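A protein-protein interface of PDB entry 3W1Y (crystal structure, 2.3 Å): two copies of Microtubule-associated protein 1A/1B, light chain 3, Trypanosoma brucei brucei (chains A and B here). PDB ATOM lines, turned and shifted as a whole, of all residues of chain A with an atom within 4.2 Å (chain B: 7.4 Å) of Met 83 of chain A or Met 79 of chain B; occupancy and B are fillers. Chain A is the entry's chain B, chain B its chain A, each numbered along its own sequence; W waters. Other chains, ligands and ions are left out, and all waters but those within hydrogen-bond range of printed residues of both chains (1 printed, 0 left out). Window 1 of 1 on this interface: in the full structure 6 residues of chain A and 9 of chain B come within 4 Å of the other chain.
O of Asn 108 of chain B sits at hydrogen-bond distance from N of Val 78 of chain B, 3.4 Å away. SD of Met 82 of chain B sits close to OD1 of Asn 108 of chain B, at 3.7 Å. OE2 of Glu 80 of chain B sits at hydrogen-bond distance from N of Thr 77 of chain B, 2.9 Å away. O of Asn 108 of chain B is in hydrogen-bond range of N of Met 79 of chain B (2.9 Å).
Among the printed residues, merely in contact across the chains: Met 83 of chain A with Glu 80 of chain B (2.9 Å), Glu 80 of chain A with Met 83 of chain B (3.4 Å), Met 79 of chain A with Met 79 of chain B (3.6 Å), Met 83 of chain A with Met 83 of chain B (3.6 Å), Met 79 of chain A with Asn 108 of chain B (3.7 Å), Arg 86 of chain A with Glu 80 of chain B (3.8 Å), Met 79 of chain A with Ser 109 of chain B (3.8 Å), Met 83 of chain A with Thr 77 of chain B (3.8 Å), Glu 80 of chain A with Met 79 of chain B (3.97 Å) and Met 83 of chain A with Met 79 of chain B (3.99 Å).
Printed residues of chain B within 4 Å of Glu 80 of chain A: Met 79 (3.97 Å) and Met 83 (3.4 Å). Phe 81 of chain A touches none of the printed residues of chain B. Of the printed residues of chain B, Met 83 of chain A touches Thr 77 (3.8 Å), Met 79 (3.99 Å), Glu 80 (2.9 Å) and Met 83 (3.6 Å). Of the printed residues of chain B, Arg 86 of chain A touches Glu 80 (3.8 Å). Of the printed residues of chain A, Glu 80 of chain B touches Met 83 and Arg 86. Printed residues of chain A within 4 Å of Met 83 of chain B: Glu 80 (3.4 Å) and Met 83 (3.6 Å). Of the printed residues of chain A, Ser 109 of chain B touches Met 79 (3.8 Å). Leu 112 of chain B touches none of the printed residues of chain A. The nearest printed residue of chain B that does not touch Met 83 of chain A is Asn 108 of chain B (6.6 Å). The nearest printed residue of chain B that does not touch Arg 86 of chain A is Thr 75 of chain B (5.8 Å).
Hydrophobic or aromatic side chains of chain A within 4 Å of the printed part of chain B: Met 79 and Met 83. Hydrophobic or aromatic side chains of chain B that line the printed part of chain A: Met 79 and Met 83. Among the printed residues, no Asp or Glu carboxylate lies within 4 Å of a Lys or Arg side-chain nitrogen of the other chain.
Met 79 of chain A touches its own counterpart, Met 79 of chain B. Glu 80 of chain A touches Met 79 of chain B, but with the chains exchanged Met 79 of chain A does not touch Glu 80 of chain B (6.6 Å). Glu 80 of chain A touches Met 83 of chain B, and with the chains exchanged Met 83 of chain A touches Glu 80 of chain B. Met 83 of chain A touches Met 79 of chain B, but with the chains exchanged Met 79 of chain A does not touch Met 83 of chain B (5.4 Å).
Water W1 bridges OE1 of Glu 80 of chain B and O of Met 83 of chain A.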
ATOM      1  N   MET A  79     -34.078 -11.269  14.695  1.00  0.00           N
ATOM      2  CA  MET A  79     -32.999 -10.426  15.180  1.00  0.00           C
ATOM      3  C   MET A  79     -32.298  -9.624  14.073  1.00  0.00           C
ATOM      4  O   MET A  79     -32.154  -8.412  14.187  1.00  0.00           O
ATOM      5  CB  MET A  79     -31.994 -11.274  15.948  1.00  0.00           C
ATOM      6  CG  MET A  79     -30.849 -10.487  16.524  1.00  0.00           C
ATOM      7  SD  MET A  79     -31.370  -9.408  17.849  1.00  0.00           S
ATOM      8  CE  MET A  79     -29.944  -9.660  18.902  1.00  0.00           C
ATOM      9  N   GLU A  80     -31.877 -10.298  13.015  1.00  0.00           N
ATOM     10  CA  GLU A  80     -31.272  -9.612  11.867  1.00  0.00           C
ATOM     11  C   GLU A  80     -32.179  -8.548  11.296  1.00  0.00           C
ATOM     12  O   GLU A  80     -31.750  -7.411  11.103  1.00  0.00           O
ATOM     13  CB  GLU A  80     -30.912 -10.589  10.759  1.00  0.00           C
ATOM     14  CG  GLU A  80     -29.812 -11.546  11.128  1.00  0.00           C
ATOM     15  CD  GLU A  80     -29.608 -12.574  10.039  1.00  0.00           C
ATOM     16  OE1 GLU A  80     -29.219 -12.154   8.925  1.00  0.00           O
ATOM     17  OE2 GLU A  80     -29.860 -13.784  10.284  1.00  0.00           O
ATOM     18  N   PHE A  81     -33.432  -8.930  11.039  1.00  0.00           N
ATOM     19  CA  PHE A  81     -34.477  -7.990  10.621  1.00  0.00           C
ATOM     20  C   PHE A  81     -34.642  -6.797  11.562  1.00  0.00           C
ATOM     21  O   PHE A  81     -34.656  -5.671  11.090  1.00  0.00           O
ATOM     22  CB  PHE A  81     -35.811  -8.704  10.400  1.00  0.00           C
ATOM     23  CG  PHE A  81     -36.965  -7.777  10.126  1.00  0.00           C
ATOM     24  CD1 PHE A  81     -36.923  -6.862   9.067  1.00  0.00           C
ATOM     25  CD2 PHE A  81     -38.127  -7.834  10.921  1.00  0.00           C
ATOM     26  CE1 PHE A  81     -38.012  -5.993   8.801  1.00  0.00           C
ATOM     27  CE2 PHE A  81     -39.227  -6.976  10.655  1.00  0.00           C
ATOM     28  CZ  PHE A  81     -39.164  -6.061   9.595  1.00  0.00           C
ATOM     29  N   MET A  82     -34.756  -7.027  12.874  1.00  0.00           N
ATOM     30  CA  MET A  82     -34.791  -5.896  13.846  1.00  0.00           C
ATOM     31  C   MET A  82     -33.557  -4.963  13.772  1.00  0.00           C
ATOM     32  O   MET A  82     -33.681  -3.759  13.950  1.00  0.00           O
ATOM     33  CB  MET A  82     -34.943  -6.382  15.291  1.00  0.00           C
ATOM     34  CG  MET A  82     -36.262  -7.089  15.602  1.00  0.00           C
ATOM     35  SD  MET A  82     -36.322  -7.702  17.304  1.00  0.00           S
ATOM     36  CE  MET A  82     -35.320  -9.149  17.263  1.00  0.00           C
ATOM     37  N   MET A  83     -32.376  -5.539  13.536  1.00  0.00           N
ATOM     38  CA  MET A  83     -31.152  -4.761  13.444  1.00  0.00           C
ATOM     39  C   MET A  83     -31.086  -3.944  12.141  1.00  0.00           C
ATOM     40  O   MET A  83     -30.687  -2.767  12.151  1.00  0.00           O
ATOM     41  CB  MET A  83     -29.906  -5.656  13.579  1.00  0.00           C
ATOM     42  CG  MET A  83     -29.591  -6.224  14.986  1.00  0.00           C
ATOM     43  SD  MET A  83     -29.864  -5.259  16.514  1.00  0.00           S
ATOM     44  CE  MET A  83     -29.879  -3.574  15.964  1.00  0.00           C
ATOM     45  N   ALA A  84     -31.478  -4.576  11.034  1.00  0.00           N
ATOM     46  CA  ALA A  84     -31.637  -3.884   9.745  1.00  0.00           C
ATOM     47  C   ALA A  84     -32.643  -2.745   9.860  1.00  0.00           C
ATOM     48  O   ALA A  84     -32.380  -1.639   9.418  1.00  0.00           O
ATOM     49  CB  ALA A  84     -32.065  -4.865   8.647  1.00  0.00           C
ATOM     50  N   LEU A  85     -33.788  -3.026  10.476  1.00  0.00           N
ATOM     51  CA  LEU A  85     -34.846  -2.042  10.686  1.00  0.00           C
ATOM     52  C   LEU A  85     -34.392  -0.877  11.561  1.00  0.00           C
ATOM     53  O   LEU A  85     -34.846   0.257  11.383  1.00  0.00           O
ATOM     54  CB  LEU A  85     -36.090  -2.718  11.293  1.00  0.00           C
ATOM     55  CG  LEU A  85     -37.435  -1.990  11.304  1.00  0.00           C
ATOM     56  CD1 LEU A  85     -37.976  -1.787   9.881  1.00  0.00           C
ATOM     57  CD2 LEU A  85     -38.445  -2.752  12.174  1.00  0.00           C
ATOM     58  N   ARG A  86     -33.500  -1.162  12.503  1.00  0.00           N
ATOM     59  CA  ARG A  86     -32.956  -0.140  13.401  1.00  0.00           C
ATOM     60  C   ARG A  86     -32.153   0.914  12.631  1.00  0.00           C
ATOM     61  O   ARG A  86     -32.401   2.114  12.791  1.00  0.00           O
ATOM     62  CB  ARG A  86     -32.097  -0.784  14.491  1.00  0.00           C
ATOM     63  CG  ARG A  86     -32.046   0.021  15.765  1.00  0.00           C
ATOM     64  CD  ARG A  86     -30.808  -0.310  16.591  1.00  0.00           C
ATOM     65  NE  ARG A  86     -30.412   0.798  17.454  1.00  0.00           N
ATOM     66  CZ  ARG A  86     -29.770   1.889  17.037  1.00  0.00           C
ATOM     67  NH1 ARG A  86     -29.441   2.046  15.760  1.00  0.00           N
ATOM     68  NH2 ARG A  86     -29.455   2.838  17.903  1.00  0.00           N
ATOM     69  N   GLN A  87     -31.208   0.455  11.800  1.00  0.00           N
ATOM     70  CA  GLN A  87     -30.451   1.312  10.865  1.00  0.00           C
ATOM     71  C   GLN A  87     -31.372   2.130   9.971  1.00  0.00           C
ATOM     72  O   GLN A  87     -31.229   3.343   9.845  1.00  0.00           O
ATOM     73  CB  GLN A  87     -29.570   0.464   9.949  1.00  0.00           C
ATOM     74  CG  GLN A  87     -28.336  -0.122  10.590  1.00  0.00           C
ATOM     75  CD  GLN A  87     -27.428  -0.790   9.571  1.00  0.00           C
ATOM     76  OE1 GLN A  87     -27.872  -1.176   8.479  1.00  0.00           O
ATOM     77  NE2 GLN A  87     -26.144  -0.926   9.916  1.00  0.00           N
ATOM     78  N   THR B  75     -22.846   0.524  22.539  1.00  0.00           N
ATOM     79  CA  THR B  75     -24.233   0.042  22.594  1.00  0.00           C
ATOM     80  C   THR B  75     -24.653  -0.921  21.436  1.00  0.00           C
ATOM     81  O   THR B  75     -25.705  -1.575  21.533  1.00  0.00           O
ATOM     82  CB  THR B  75     -25.232   1.220  22.667  1.00  0.00           C
ATOM     83  OG1 THR B  75     -24.966   2.116  21.583  1.00  0.00           O
ATOM     84  CG2 THR B  75     -25.090   1.987  23.992  1.00  0.00           C
ATOM     85  N   ALA B  76     -23.860  -0.995  20.362  1.00  0.00           N
ATOM     86  CA  ALA B  76     -24.068  -2.006  19.321  1.00  0.00           C
ATOM     87  C   ALA B  76     -24.072  -3.412  19.920  1.00  0.00           C
ATOM     88  O   ALA B  76     -23.358  -3.688  20.861  1.00  0.00           O
ATOM     89  CB  ALA B  76     -22.972  -1.901  18.225  1.00  0.00           C
ATOM     90  N   THR B  77     -24.882  -4.301  19.374  1.00  0.00           N
ATOM     91  CA  THR B  77     -24.864  -5.709  19.807  1.00  0.00           C
ATOM     92  C   THR B  77     -23.863  -6.555  19.018  1.00  0.00           C
ATOM     93  O   THR B  77     -23.378  -6.131  17.967  1.00  0.00           O
ATOM     94  CB  THR B  77     -26.210  -6.338  19.632  1.00  0.00           C
ATOM     95  OG1 THR B  77     -26.580  -6.206  18.266  1.00  0.00           O
ATOM     96  CG2 THR B  77     -27.240  -5.632  20.511  1.00  0.00           C
ATOM     97  N   VAL B  78     -23.580  -7.763  19.534  1.00  0.00           N
ATOM     98  CA  VAL B  78     -22.809  -8.766  18.814  1.00  0.00           C
ATOM     99  C   VAL B  78     -23.379  -9.012  17.414  1.00  0.00           C
ATOM    100  O   VAL B  78     -22.635  -9.086  16.445  1.00  0.00           O
ATOM    101  CB  VAL B  78     -22.680 -10.083  19.621  1.00  0.00           C
ATOM    102  CG1 VAL B  78     -22.169 -11.205  18.765  1.00  0.00           C
ATOM    103  CG2 VAL B  78     -21.739  -9.902  20.792  1.00  0.00           C
ATOM    104  N   MET B  79     -24.700  -9.117  17.302  1.00  0.00           N
ATOM    105  CA  MET B  79     -25.329  -9.326  16.007  1.00  0.00           C
ATOM    106  C   MET B  79     -24.993  -8.212  15.000  1.00  0.00           C
ATOM    107  O   MET B  79     -24.727  -8.482  13.825  1.00  0.00           O
ATOM    108  CB  MET B  79     -26.863  -9.503  16.187  1.00  0.00           C
ATOM    109  CG  MET B  79     -27.635  -9.702  14.875  1.00  0.00           C
ATOM    110  SD  MET B  79     -27.147 -11.265  14.062  1.00  0.00           S
ATOM    111  CE  MET B  79     -28.224 -12.374  14.964  1.00  0.00           C
ATOM    112  N   GLU B  80     -25.041  -6.964  15.459  1.00  0.00           N
ATOM    113  CA  GLU B  80     -24.735  -5.821  14.591  1.00  0.00           C
ATOM    114  C   GLU B  80     -23.301  -5.882  14.089  1.00  0.00           C
ATOM    115  O   GLU B  80     -23.046  -5.672  12.906  1.00  0.00           O
ATOM    116  CB  GLU B  80     -25.020  -4.480  15.298  1.00  0.00           C
ATOM    117  CG  GLU B  80     -26.482  -4.069  15.185  1.00  0.00           C
ATOM    118  CD  GLU B  80     -26.897  -2.950  16.158  1.00  0.00           C
ATOM    119  OE1 GLU B  80     -27.462  -1.937  15.678  1.00  0.00           O
ATOM    120  OE2 GLU B  80     -26.695  -3.091  17.389  1.00  0.00           O
ATOM    121  N   PHE B  81     -22.375  -6.178  14.998  1.00  0.00           N
ATOM    122  CA  PHE B  81     -20.993  -6.452  14.633  1.00  0.00           C
ATOM    123  C   PHE B  81     -20.890  -7.545  13.577  1.00  0.00           C
ATOM    124  O   PHE B  81     -20.199  -7.378  12.577  1.00  0.00           O
ATOM    125  CB  PHE B  81     -20.174  -6.825  15.879  1.00  0.00           C
ATOM    126  CG  PHE B  81     -18.831  -7.418  15.575  1.00  0.00           C
ATOM    127  CD1 PHE B  81     -17.938  -6.780  14.743  1.00  0.00           C
ATOM    128  CD2 PHE B  81     -18.454  -8.620  16.149  1.00  0.00           C
ATOM    129  CE1 PHE B  81     -16.714  -7.332  14.468  1.00  0.00           C
ATOM    130  CE2 PHE B  81     -17.199  -9.176  15.877  1.00  0.00           C
ATOM    131  CZ  PHE B  81     -16.348  -8.531  15.033  1.00  0.00           C
ATOM    132  N   MET B  82     -21.580  -8.651  13.798  1.00  0.00           N
ATOM    133  CA  MET B  82     -21.532  -9.756  12.867  1.00  0.00           C
ATOM    134  C   MET B  82     -22.074  -9.397  11.489  1.00  0.00           C
ATOM    135  O   MET B  82     -21.538  -9.847  10.476  1.00  0.00           O
ATOM    136  CB  MET B  82     -22.275 -10.950  13.424  1.00  0.00           C
ATOM    137  CG  MET B  82     -21.455 -11.838  14.317  1.00  0.00           C
ATOM    138  SD  MET B  82     -22.647 -12.877  15.167  1.00  0.00           S
ATOM    139  CE  MET B  82     -23.034 -14.038  13.864  1.00  0.00           C
ATOM    140  N   MET B  83     -23.125  -8.583  11.456  1.00  0.00           N
ATOM    141  CA  MET B  83     -23.648  -8.059  10.193  1.00  0.00           C
ATOM    142  C   MET B  83     -22.677  -7.101   9.539  1.00  0.00           C
ATOM    143  O   MET B  83     -22.512  -7.171   8.342  1.00  0.00           O
ATOM    144  CB  MET B  83     -25.021  -7.401  10.357  1.00  0.00           C
ATOM    145  CG  MET B  83     -26.062  -8.368  10.921  1.00  0.00           C
ATOM    146  SD  MET B  83     -27.510  -7.465  11.510  1.00  0.00           S
ATOM    147  CE  MET B  83     -28.495  -7.445   9.969  1.00  0.00           C
ATOM    148  N   ALA B  84     -22.012  -6.236  10.309  1.00  0.00           N
ATOM    149  CA  ALA B  84     -20.946  -5.400   9.738  1.00  0.00           C
ATOM    150  C   ALA B  84     -19.790  -6.237   9.104  1.00  0.00           C
ATOM    151  O   ALA B  84     -19.271  -5.891   8.036  1.00  0.00           O
ATOM    152  CB  ALA B  84     -20.417  -4.419  10.772  1.00  0.00           C
ATOM    153  N   LEU B  85     -19.432  -7.345   9.756  1.00  0.00           N
ATOM    154  CA  LEU B  85     -18.353  -8.232   9.300  1.00  0.00           C
ATOM    155  C   LEU B  85     -18.764  -8.975   8.025  1.00  0.00           C
ATOM    156  O   LEU B  85     -17.974  -9.117   7.106  1.00  0.00           O
ATOM    157  CB  LEU B  85     -17.908  -9.205  10.410  1.00  0.00           C
ATOM    158  CG  LEU B  85     -16.751 -10.215  10.202  1.00  0.00           C
ATOM    159  CD1 LEU B  85     -15.379  -9.580   9.798  1.00  0.00           C
ATOM    160  CD2 LEU B  85     -16.585 -11.011  11.488  1.00  0.00           C
ATOM    161  N   VAL B  99     -18.334 -15.578  15.224  1.00  0.00           N
ATOM    162  CA  VAL B  99     -17.232 -14.919  15.935  1.00  0.00           C
ATOM    163  C   VAL B  99     -16.981 -15.455  17.360  1.00  0.00           C
ATOM    164  O   VAL B  99     -17.907 -15.880  18.047  1.00  0.00           O
ATOM    165  CB  VAL B  99     -17.397 -13.367  15.990  1.00  0.00           C
ATOM    166  CG1 VAL B  99     -17.368 -12.761  14.579  1.00  0.00           C
ATOM    167  CG2 VAL B  99     -18.664 -12.963  16.720  1.00  0.00           C
ATOM    168  N   PRO B 106     -19.912 -15.367  21.817  1.00  0.00           N
ATOM    169  CA  PRO B 106     -20.747 -14.472  22.614  1.00  0.00           C
ATOM    170  C   PRO B 106     -22.238 -14.520  22.207  1.00  0.00           C
ATOM    171  O   PRO B 106     -22.556 -14.843  21.059  1.00  0.00           O
ATOM    172  CB  PRO B 106     -20.146 -13.097  22.332  1.00  0.00           C
ATOM    173  CG  PRO B 106     -19.553 -13.232  20.938  1.00  0.00           C
ATOM    174  CD  PRO B 106     -19.068 -14.641  20.845  1.00  0.00           C
ATOM    175  N   PRO B 107     -23.149 -14.237  23.164  1.00  0.00           N
ATOM    176  CA  PRO B 107     -24.572 -14.142  22.816  1.00  0.00           C
ATOM    177  C   PRO B 107     -24.786 -12.979  21.830  1.00  0.00           C
ATOM    178  O   PRO B 107     -24.143 -11.928  21.969  1.00  0.00           O
ATOM    179  CB  PRO B 107     -25.267 -13.832  24.163  1.00  0.00           C
ATOM    180  CG  PRO B 107     -24.248 -14.095  25.234  1.00  0.00           C
ATOM    181  CD  PRO B 107     -22.892 -13.992  24.600  1.00  0.00           C
ATOM    182  N   ASN B 108     -25.675 -13.191  20.861  1.00  0.00           N
ATOM    183  CA  ASN B 108     -26.023 -12.193  19.837  1.00  0.00           C
ATOM    184  C   ASN B 108     -26.534 -10.841  20.315  1.00  0.00           C
ATOM    185  O   ASN B 108     -26.321  -9.824  19.631  1.00  0.00           O
ATOM    186  CB  ASN B 108     -27.034 -12.774  18.859  1.00  0.00           C
ATOM    187  CG  ASN B 108     -26.393 -13.728  17.914  1.00  0.00           C
ATOM    188  OD1 ASN B 108     -25.169 -13.726  17.784  1.00  0.00           O
ATOM    189  ND2 ASN B 108     -27.188 -14.563  17.261  1.00  0.00           N
ATOM    190  N   SER B 109     -27.193 -10.842  21.478  1.00  0.00           N
ATOM    191  CA  SER B 109     -27.773  -9.635  22.067  1.00  0.00           C
ATOM    192  C   SER B 109     -26.846  -8.959  23.041  1.00  0.00           C
ATOM    193  O   SER B 109     -27.204  -7.952  23.607  1.00  0.00           O
ATOM    194  CB  SER B 109     -29.087  -9.965  22.775  1.00  0.00           C
ATOM    195  OG  SER B 109     -28.887 -10.911  23.828  1.00  0.00           O
ATOM    196  N   ALA B 110     -25.660  -9.509  23.266  1.00  0.00           N
ATOM    197  CA  ALA B 110     -24.682  -8.846  24.131  1.00  0.00           C
ATOM    198  C   ALA B 110     -24.198  -7.534  23.491  1.00  0.00           C
ATOM    199  O   ALA B 110     -24.095  -7.440  22.271  1.00  0.00           O
ATOM    200  CB  ALA B 110     -23.508  -9.782  24.428  1.00  0.00           C
ATOM    201  N   LEU B 112     -21.264  -4.839  22.717  1.00  0.00           N
ATOM    202  CA  LEU B 112     -19.808  -4.727  22.530  1.00  0.00           C
ATOM    203  C   LEU B 112     -19.110  -4.063  23.715  1.00  0.00           C
ATOM    204  O   LEU B 112     -18.041  -4.511  24.128  1.00  0.00           O
ATOM    205  CB  LEU B 112     -19.484  -3.955  21.242  1.00  0.00           C
ATOM    206  CG  LEU B 112     -20.108  -4.549  19.983  1.00  0.00           C
ATOM    207  CD1 LEU B 112     -19.694  -3.839  18.680  1.00  0.00           C
ATOM    208  CD2 LEU B 112     -19.798  -6.045  19.911  1.00  0.00           C
HETATM  209  O   HOH W   1     -28.336  -1.493  13.285  1.00  0.00           O
